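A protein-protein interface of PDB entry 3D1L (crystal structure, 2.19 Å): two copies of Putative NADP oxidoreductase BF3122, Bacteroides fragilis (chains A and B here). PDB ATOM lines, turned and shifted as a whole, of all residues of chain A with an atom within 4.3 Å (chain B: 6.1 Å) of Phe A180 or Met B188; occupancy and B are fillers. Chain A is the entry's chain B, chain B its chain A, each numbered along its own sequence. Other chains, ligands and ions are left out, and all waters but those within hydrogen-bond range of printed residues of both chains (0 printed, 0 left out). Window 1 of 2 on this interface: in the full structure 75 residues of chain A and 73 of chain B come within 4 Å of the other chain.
The backbone carbonyl oxygen (O) of Ala A177 sits at hydrogen-bond distance from the side-chain hydroxyl (OG1) of Thr A181 (3.0 Å). The backbone carbonyl oxygen (O) of Val A179 lies within hydrogen-bond range of the backbone NH (N) of Phe A184. O of Phe A180 lies within hydrogen-bond range of OG1 of Thr A185 (3.3 Å). The backbone carbonyl oxygen (O) of Thr A181 is in hydrogen-bond range of the side-chain hydroxyl (OG1) of Thr A185 (3.0 Å).
Among the printed residues, pairs that only touch across the chains: Leu A176 with Tyr B255 (3.8 Å), Ala A177 with Ala B192 (3.7 Å), Val A179 with Tyr B255 (3.8 Å), Phe A180 with Met B188 (3.4 Å), Phe A180 with Leu B191 (3.7 Å), Phe A180 with Leu B195 (3.7 Å), Phe A180 with Met B251 (3.7 Å), Phe A180 with Tyr B255 (3.9 Å), Thr A181 with Ala B192 (3.1 Å), Phe A184 with Met B188 (3.7 Å), Phe A184 with Tyr B255 (3.5 Å), Phe A184 with Leu B258 (3.7 Å), Thr A185 with Thr B185 (3.5 Å), Thr A185 with Met B188 (3.4 Å), Thr A185 with Tyr B189 (3.8 Å), Leu A258 with Phe B184 (3.7 Å) and Leu A258 with Met B188 (3.3 Å).
Phe A180 touches just these residues of chain B: Met B188 (3.4 Å), Leu B191 (3.7 Å), Leu B195 (3.7 Å), Met B251 (3.7 Å) and Tyr B255 (3.9 Å). Printed residues of chain B within 4 Å of Thr A185: Thr B185 (3.5 Å), Met B188 (3.4 Å) and Tyr B189 (3.8 Å). Printed residues of chain A within 4 Å of Thr B185: Thr A185 (3.5 Å). Met B188 touches just these residues of chain A: Phe A180 (3.4 Å), Phe A184 (3.7 Å), Thr A185 (3.4 Å) and Leu A258 (3.3 Å). Ala B190 touches none of the printed residues of chain A. Of the printed residues of chain A, Leu B258 touches Phe A184 (3.7 Å). The nearest residue of chain B that does not touch Phe A180 is Leu B245 (4.1 Å). The nearest printed residue of chain A that does not touch Met B188 is Thr A181 (4.7 Å). The nearest printed residue of chain B that does not touch Ala A177 is Leu B195 (4.5 Å).
Of the 17 printed residues of chain B, 10 touch a printed residue of chain A. Hydrophobic or aromatic side chains of chain B within 4 Å of the printed part of chain A: Phe B184, Met B188, Tyr B189, Leu B191, Ala B192, Leu B195, Met B251, Tyr B255 and Leu B258. Hydrophobic or aromatic side chains of chain A that line the printed part of chain B: Leu A176, Val A179, Phe A180, Phe A184 and Leu A258. Among the printed residues, 17 pairs touch across the chains.
Phe A184 touches Leu B258, and with the chains exchanged Leu A258 touches Phe B184. Thr A185 touches its own counterpart, Thr B185. Of the 17 pairs that touch across the chains among the printed residues, 3 have their exchanged pair printed and touching as well.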
ATOM      1  N   LEU A 176     -15.775  31.295  -8.496  1.00  0.00           N
ATOM      2  CA  LEU A 176     -16.380  30.167  -9.212  1.00  0.00           C
ATOM      3  C   LEU A 176     -17.142  30.640 -10.439  1.00  0.00           C
ATOM      4  O   LEU A 176     -16.983  30.095 -11.536  1.00  0.00           O
ATOM      5  CB  LEU A 176     -17.286  29.325  -8.298  1.00  0.00           C
ATOM      6  CG  LEU A 176     -18.168  28.254  -8.970  1.00  0.00           C
ATOM      7  CD1 LEU A 176     -17.366  27.056  -9.501  1.00  0.00           C
ATOM      8  CD2 LEU A 176     -19.249  27.769  -8.020  1.00  0.00           C
ATOM      9  N   ALA A 177     -17.967  31.667 -10.255  1.00  0.00           N
ATOM     10  CA  ALA A 177     -18.691  32.270 -11.374  1.00  0.00           C
ATOM     11  C   ALA A 177     -17.740  32.843 -12.446  1.00  0.00           C
ATOM     12  O   ALA A 177     -18.019  32.780 -13.638  1.00  0.00           O
ATOM     13  CB  ALA A 177     -19.654  33.346 -10.841  1.00  0.00           C
ATOM     14  N   ALA A 178     -16.611  33.392 -12.011  1.00  0.00           N
ATOM     15  CA  ALA A 178     -15.600  33.977 -12.918  1.00  0.00           C
ATOM     16  C   ALA A 178     -14.910  32.895 -13.714  1.00  0.00           C
ATOM     17  O   ALA A 178     -14.404  33.156 -14.793  1.00  0.00           O
ATOM     18  CB  ALA A 178     -14.543  34.784 -12.112  1.00  0.00           C
ATOM     19  N   VAL A 179     -14.810  31.686 -13.167  1.00  0.00           N
ATOM     20  CA  VAL A 179     -14.166  30.639 -13.966  1.00  0.00           C
ATOM     21  C   VAL A 179     -15.038  30.329 -15.197  1.00  0.00           C
ATOM     22  O   VAL A 179     -14.515  30.208 -16.328  1.00  0.00           O
ATOM     23  CB  VAL A 179     -13.818  29.350 -13.152  1.00  0.00           C
ATOM     24  CG1 VAL A 179     -13.393  28.217 -14.102  1.00  0.00           C
ATOM     25  CG2 VAL A 179     -12.739  29.617 -12.121  1.00  0.00           C
ATOM     26  N   PHE A 180     -16.356  30.205 -14.991  1.00  0.00           N
ATOM     27  CA  PHE A 180     -17.295  30.096 -16.132  1.00  0.00           C
ATOM     28  C   PHE A 180     -17.194  31.294 -17.034  1.00  0.00           C
ATOM     29  O   PHE A 180     -17.043  31.189 -18.257  1.00  0.00           O
ATOM     30  CB  PHE A 180     -18.747  29.968 -15.634  1.00  0.00           C
ATOM     31  CG  PHE A 180     -19.069  28.613 -15.084  1.00  0.00           C
ATOM     32  CD1 PHE A 180     -19.518  27.603 -15.930  1.00  0.00           C
ATOM     33  CD2 PHE A 180     -18.868  28.328 -13.736  1.00  0.00           C
ATOM     34  CE1 PHE A 180     -19.805  26.324 -15.423  1.00  0.00           C
ATOM     35  CE2 PHE A 180     -19.155  27.052 -13.222  1.00  0.00           C
ATOM     36  CZ  PHE A 180     -19.619  26.052 -14.078  1.00  0.00           C
ATOM     37  N   THR A 181     -17.304  32.461 -16.421  1.00  0.00           N
ATOM     38  CA  THR A 181     -17.392  33.688 -17.196  1.00  0.00           C
ATOM     39  C   THR A 181     -16.172  33.940 -18.058  1.00  0.00           C
ATOM     40  O   THR A 181     -16.317  34.418 -19.188  1.00  0.00           O
ATOM     41  CB  THR A 181     -17.658  34.903 -16.308  1.00  0.00           C
ATOM     42  OG1 THR A 181     -18.941  34.726 -15.698  1.00  0.00           O
ATOM     43  CG2 THR A 181     -17.688  36.158 -17.153  1.00  0.00           C
ATOM     44  N   CYS A 182     -14.985  33.668 -17.524  1.00  0.00           N
ATOM     45  CA  CYS A 182     -13.736  34.045 -18.213  1.00  0.00           C
ATOM     46  C   CYS A 182     -12.983  32.857 -18.785  1.00  0.00           C
ATOM     47  O   CYS A 182     -12.549  32.872 -19.945  1.00  0.00           O
ATOM     48  CB  CYS A 182     -12.759  34.711 -17.239  1.00  0.00           C
ATOM     49  SG  CYS A 182     -13.244  36.298 -16.508  1.00  0.00           S
ATOM     50  N   PHE A 184     -13.731  29.432 -19.036  1.00  0.00           N
ATOM     51  CA  PHE A 184     -14.449  28.511 -19.929  1.00  0.00           C
ATOM     52  C   PHE A 184     -14.876  29.215 -21.232  1.00  0.00           C
ATOM     53  O   PHE A 184     -14.932  28.608 -22.292  1.00  0.00           O
ATOM     54  CB  PHE A 184     -15.664  27.880 -19.243  1.00  0.00           C
ATOM     55  CG  PHE A 184     -15.315  27.014 -18.045  1.00  0.00           C
ATOM     56  CD1 PHE A 184     -14.003  26.607 -17.813  1.00  0.00           C
ATOM     57  CD2 PHE A 184     -16.310  26.584 -17.168  1.00  0.00           C
ATOM     58  CE1 PHE A 184     -13.692  25.800 -16.715  1.00  0.00           C
ATOM     59  CE2 PHE A 184     -16.008  25.764 -16.071  1.00  0.00           C
ATOM     60  CZ  PHE A 184     -14.695  25.372 -15.848  1.00  0.00           C
ATOM     61  N   THR A 185     -15.212  30.493 -21.120  1.00  0.00           N
ATOM     62  CA  THR A 185     -15.555  31.303 -22.277  1.00  0.00           C
ATOM     63  C   THR A 185     -14.370  31.412 -23.223  1.00  0.00           C
ATOM     64  O   THR A 185     -14.503  31.163 -24.423  1.00  0.00           O
ATOM     65  CB  THR A 185     -16.014  32.696 -21.846  1.00  0.00           C
ATOM     66  OG1 THR A 185     -17.339  32.603 -21.279  1.00  0.00           O
ATOM     67  CG2 THR A 185     -16.066  33.636 -23.088  1.00  0.00           C
ATOM     68  N   LEU A 258     -22.948  20.537 -23.616  1.00  0.00           N
ATOM     69  CA  LEU A 258     -23.268  21.971 -23.662  1.00  0.00           C
ATOM     70  C   LEU A 258     -24.621  22.217 -24.348  1.00  0.00           C
ATOM     71  O   LEU A 258     -25.428  23.026 -23.884  1.00  0.00           O
ATOM     72  CB  LEU A 258     -22.134  22.774 -24.336  1.00  0.00           C
ATOM     73  CG  LEU A 258     -20.838  22.893 -23.511  1.00  0.00           C
ATOM     74  CD1 LEU A 258     -19.583  23.233 -24.364  1.00  0.00           C
ATOM     75  CD2 LEU A 258     -20.965  23.901 -22.359  1.00  0.00           C
ATOM     76  N   ASN B 183     -22.938  30.541 -28.963  1.00  0.00           N
ATOM     77  CA  ASN B 183     -23.965  29.843 -28.209  1.00  0.00           C
ATOM     78  C   ASN B 183     -23.406  29.309 -26.899  1.00  0.00           C
ATOM     79  O   ASN B 183     -24.009  29.487 -25.830  1.00  0.00           O
ATOM     80  CB  ASN B 183     -24.595  28.719 -29.025  1.00  0.00           C
ATOM     81  CG  ASN B 183     -25.215  29.204 -30.338  1.00  0.00           C
ATOM     82  OD1 ASN B 183     -25.339  28.431 -31.273  1.00  0.00           O
ATOM     83  ND2 ASN B 183     -25.630  30.461 -30.396  1.00  0.00           N
ATOM     84  N   PHE B 184     -22.246  28.661 -27.006  1.00  0.00           N
ATOM     85  CA  PHE B 184     -21.609  28.012 -25.860  1.00  0.00           C
ATOM     86  C   PHE B 184     -21.014  29.065 -24.911  1.00  0.00           C
ATOM     87  O   PHE B 184     -21.037  28.889 -23.698  1.00  0.00           O
ATOM     88  CB  PHE B 184     -20.560  26.974 -26.307  1.00  0.00           C
ATOM     89  CG  PHE B 184     -21.144  25.739 -27.006  1.00  0.00           C
ATOM     90  CD1 PHE B 184     -22.517  25.458 -26.976  1.00  0.00           C
ATOM     91  CD2 PHE B 184     -20.311  24.856 -27.669  1.00  0.00           C
ATOM     92  CE1 PHE B 184     -23.038  24.323 -27.622  1.00  0.00           C
ATOM     93  CE2 PHE B 184     -20.820  23.718 -28.299  1.00  0.00           C
ATOM     94  CZ  PHE B 184     -22.195  23.450 -28.270  1.00  0.00           C
ATOM     95  N   THR B 185     -20.512  30.157 -25.473  1.00  0.00           N
ATOM     96  CA  THR B 185     -20.017  31.296 -24.685  1.00  0.00           C
ATOM     97  C   THR B 185     -21.132  31.981 -23.862  1.00  0.00           C
ATOM     98  O   THR B 185     -20.989  32.204 -22.658  1.00  0.00           O
ATOM     99  CB  THR B 185     -19.340  32.316 -25.607  1.00  0.00           C
ATOM    100  OG1 THR B 185     -18.073  31.791 -26.016  1.00  0.00           O
ATOM    101  CG2 THR B 185     -19.083  33.586 -24.863  1.00  0.00           C
ATOM    102  N   ASN B 186     -22.240  32.305 -24.528  1.00  0.00           N
ATOM    103  CA  ASN B 186     -23.393  32.842 -23.837  1.00  0.00           C
ATOM    104  C   ASN B 186     -23.902  31.895 -22.763  1.00  0.00           C
ATOM    105  O   ASN B 186     -24.310  32.351 -21.690  1.00  0.00           O
ATOM    106  CB  ASN B 186     -24.527  33.204 -24.796  1.00  0.00           C
ATOM    107  CG  ASN B 186     -25.634  33.981 -24.097  1.00  0.00           C
ATOM    108  OD1 ASN B 186     -25.542  35.198 -23.931  1.00  0.00           O
ATOM    109  ND2 ASN B 186     -26.680  33.282 -23.685  1.00  0.00           N
ATOM    110  N   HIS B 187     -23.859  30.589 -23.020  1.00  0.00           N
ATOM    111  CA  HIS B 187     -24.259  29.625 -21.980  1.00  0.00           C
ATOM    112  C   HIS B 187     -23.346  29.706 -20.756  1.00  0.00           C
ATOM    113  O   HIS B 187     -23.811  29.491 -19.628  1.00  0.00           O
ATOM    114  CB  HIS B 187     -24.304  28.187 -22.497  1.00  0.00           C
ATOM    115  CG  HIS B 187     -24.948  27.223 -21.537  1.00  0.00           C
ATOM    116  ND1 HIS B 187     -26.187  27.447 -20.972  1.00  0.00           N
ATOM    117  CD2 HIS B 187     -24.523  26.034 -21.048  1.00  0.00           C
ATOM    118  CE1 HIS B 187     -26.492  26.446 -20.164  1.00  0.00           C
ATOM    119  NE2 HIS B 187     -25.496  25.580 -20.187  1.00  0.00           N
ATOM    120  N   MET B 188     -22.060  30.024 -20.968  1.00  0.00           N
ATOM    121  CA  MET B 188     -21.141  30.164 -19.836  1.00  0.00           C
ATOM    122  C   MET B 188     -21.590  31.332 -18.986  1.00  0.00           C
ATOM    123  O   MET B 188     -21.616  31.215 -17.758  1.00  0.00           O
ATOM    124  CB  MET B 188     -19.671  30.313 -20.277  1.00  0.00           C
ATOM    125  CG  MET B 188     -19.082  29.110 -21.041  1.00  0.00           C
ATOM    126  SD  MET B 188     -19.211  27.433 -20.031  1.00  0.00           S
ATOM    127  CE  MET B 188     -20.845  26.811 -20.731  1.00  0.00           C
ATOM    128  N   TYR B 189     -21.963  32.442 -19.637  1.00  0.00           N
ATOM    129  CA  TYR B 189     -22.534  33.616 -18.945  1.00  0.00           C
ATOM    130  C   TYR B 189     -23.803  33.229 -18.168  1.00  0.00           C
ATOM    131  O   TYR B 189     -23.994  33.673 -17.028  1.00  0.00           O
ATOM    132  CB  TYR B 189     -22.919  34.765 -19.911  1.00  0.00           C
ATOM    133  CG  TYR B 189     -21.895  35.242 -20.916  1.00  0.00           C
ATOM    134  CD1 TYR B 189     -20.513  35.151 -20.676  1.00  0.00           C
ATOM    135  CD2 TYR B 189     -22.315  35.861 -22.106  1.00  0.00           C
ATOM    136  CE1 TYR B 189     -19.573  35.639 -21.628  1.00  0.00           C
ATOM    137  CE2 TYR B 189     -21.402  36.330 -23.047  1.00  0.00           C
ATOM    138  CZ  TYR B 189     -20.035  36.225 -22.789  1.00  0.00           C
ATOM    139  OH  TYR B 189     -19.153  36.717 -23.718  1.00  0.00           O
ATOM    140  N   ALA B 190     -24.665  32.428 -18.809  1.00  0.00           N
ATOM    141  CA  ALA B 190     -25.902  31.932 -18.184  1.00  0.00           C
ATOM    142  C   ALA B 190     -25.615  31.095 -16.951  1.00  0.00           C
ATOM    143  O   ALA B 190     -26.256  31.291 -15.930  1.00  0.00           O
ATOM    144  CB  ALA B 190     -26.764  31.131 -19.199  1.00  0.00           C
ATOM    145  N   LEU B 191     -24.673  30.151 -17.030  1.00  0.00           N
ATOM    146  CA  LEU B 191     -24.333  29.339 -15.830  1.00  0.00           C
ATOM    147  C   LEU B 191     -23.724  30.170 -14.681  1.00  0.00           C
ATOM    148  O   LEU B 191     -23.968  29.903 -13.509  1.00  0.00           O
ATOM    149  CB  LEU B 191     -23.406  28.195 -16.191  1.00  0.00           C
ATOM    150  CG  LEU B 191     -23.959  27.157 -17.171  1.00  0.00           C
ATOM    151  CD1 LEU B 191     -22.839  26.196 -17.590  1.00  0.00           C
ATOM    152  CD2 LEU B 191     -25.186  26.420 -16.542  1.00  0.00           C
ATOM    153  N   ALA B 192     -22.948  31.192 -15.034  1.00  0.00           N
ATOM    154  CA  ALA B 192     -22.421  32.125 -14.072  1.00  0.00           C
ATOM    155  C   ALA B 192     -23.576  32.850 -13.377  1.00  0.00           C
ATOM    156  O   ALA B 192     -23.562  33.020 -12.164  1.00  0.00           O
ATOM    157  CB  ALA B 192     -21.488  33.131 -14.763  1.00  0.00           C
ATOM    158  N   ALA B 193     -24.559  33.287 -14.164  1.00  0.00           N
ATOM    159  CA  ALA B 193     -25.701  34.031 -13.660  1.00  0.00           C
ATOM    160  C   ALA B 193     -26.531  33.173 -12.697  1.00  0.00           C
ATOM    161  O   ALA B 193     -27.023  33.687 -11.682  1.00  0.00           O
ATOM    162  CB  ALA B 193     -26.564  34.515 -14.804  1.00  0.00           C
ATOM    163  N   LEU B 195     -25.428  30.769 -10.860  1.00  0.00           N
ATOM    164  CA  LEU B 195     -24.647  30.671  -9.623  1.00  0.00           C
ATOM    165  C   LEU B 195     -24.740  31.934  -8.775  1.00  0.00           C
ATOM    166  O   LEU B 195     -25.051  31.870  -7.587  1.00  0.00           O
ATOM    167  CB  LEU B 195     -23.186  30.323  -9.929  1.00  0.00           C
ATOM    168  CG  LEU B 195     -22.961  28.915 -10.496  1.00  0.00           C
ATOM    169  CD1 LEU B 195     -21.593  28.813 -11.141  1.00  0.00           C
ATOM    170  CD2 LEU B 195     -23.158  27.841  -9.397  1.00  0.00           C
ATOM    171  N   LEU B 245     -20.442  22.761  -6.679  1.00  0.00           N
ATOM    172  CA  LEU B 245     -21.372  22.419  -7.748  1.00  0.00           C
ATOM    173  C   LEU B 245     -22.052  21.058  -7.527  1.00  0.00           C
ATOM    174  O   LEU B 245     -22.824  20.619  -8.371  1.00  0.00           O
ATOM    175  CB  LEU B 245     -20.623  22.389  -9.084  1.00  0.00           C
ATOM    176  CG  LEU B 245     -20.064  23.699  -9.629  1.00  0.00           C
ATOM    177  CD1 LEU B 245     -19.305  23.424 -10.920  1.00  0.00           C
ATOM    178  CD2 LEU B 245     -21.202  24.712  -9.842  1.00  0.00           C
ATOM    179  N   MET B 251     -23.929  20.452 -14.250  1.00  0.00           N
ATOM    180  CA  MET B 251     -23.002  21.585 -14.278  1.00  0.00           C
ATOM    181  C   MET B 251     -21.625  21.222 -13.751  1.00  0.00           C
ATOM    182  O   MET B 251     -20.623  21.748 -14.211  1.00  0.00           O
ATOM    183  CB  MET B 251     -23.553  22.787 -13.511  1.00  0.00           C
ATOM    184  CG  MET B 251     -22.785  24.071 -13.815  1.00  0.00           C
ATOM    185  SD  MET B 251     -23.388  25.575 -12.803  1.00  0.00           S
ATOM    186  CE  MET B 251     -25.287  25.262 -12.910  1.00  0.00           C
ATOM    187  N   LEU B 254     -19.669  19.330 -16.452  1.00  0.00           N
ATOM    188  CA  LEU B 254     -19.266  20.372 -17.391  1.00  0.00           C
ATOM    189  C   LEU B 254     -17.991  21.073 -16.904  1.00  0.00           C
ATOM    190  O   LEU B 254     -17.024  21.183 -17.643  1.00  0.00           O
ATOM    191  CB  LEU B 254     -20.415  21.369 -17.510  1.00  0.00           C
ATOM    192  CG  LEU B 254     -20.985  21.711 -18.885  1.00  0.00           C
ATOM    193  CD1 LEU B 254     -20.972  20.535 -19.879  1.00  0.00           C
ATOM    194  CD2 LEU B 254     -22.381  22.321 -18.742  1.00  0.00           C
ATOM    195  N   TYR B 255     -17.996  21.511 -15.645  1.00  0.00           N
ATOM    196  CA  TYR B 255     -16.825  22.157 -15.041  1.00  0.00           C
ATOM    197  C   TYR B 255     -15.623  21.238 -15.141  1.00  0.00           C
ATOM    198  O   TYR B 255     -14.525  21.661 -15.529  1.00  0.00           O
ATOM    199  CB  TYR B 255     -17.092  22.523 -13.561  1.00  0.00           C
ATOM    200  CG  TYR B 255     -15.972  23.341 -12.926  1.00  0.00           C
ATOM    201  CD1 TYR B 255     -16.133  24.712 -12.674  1.00  0.00           C
ATOM    202  CD2 TYR B 255     -14.751  22.744 -12.606  1.00  0.00           C
ATOM    203  CE1 TYR B 255     -15.086  25.465 -12.099  1.00  0.00           C
ATOM    204  CE2 TYR B 255     -13.708  23.471 -12.044  1.00  0.00           C
ATOM    205  CZ  TYR B 255     -13.872  24.830 -11.801  1.00  0.00           C
ATOM    206  OH  TYR B 255     -12.820  25.533 -11.259  1.00  0.00           O
ATOM    207  N   LEU B 258     -14.610  20.672 -18.953  1.00  0.00           N
ATOM    208  CA  LEU B 258     -14.006  21.902 -19.508  1.00  0.00           C
ATOM    209  C   LEU B 258     -12.614  22.142 -18.967  1.00  0.00           C
ATOM    210  O   LEU B 258     -11.703  22.543 -19.711  1.00  0.00           O
ATOM    211  CB  LEU B 258     -14.901  23.111 -19.272  1.00  0.00           C
ATOM    212  CG  LEU B 258     -16.170  23.096 -20.120  1.00  0.00           C
ATOM    213  CD1 LEU B 258     -17.260  23.985 -19.551  1.00  0.00           C
ATOM    214  CD2 LEU B 258     -15.829  23.495 -21.565  1.00  0.00           C
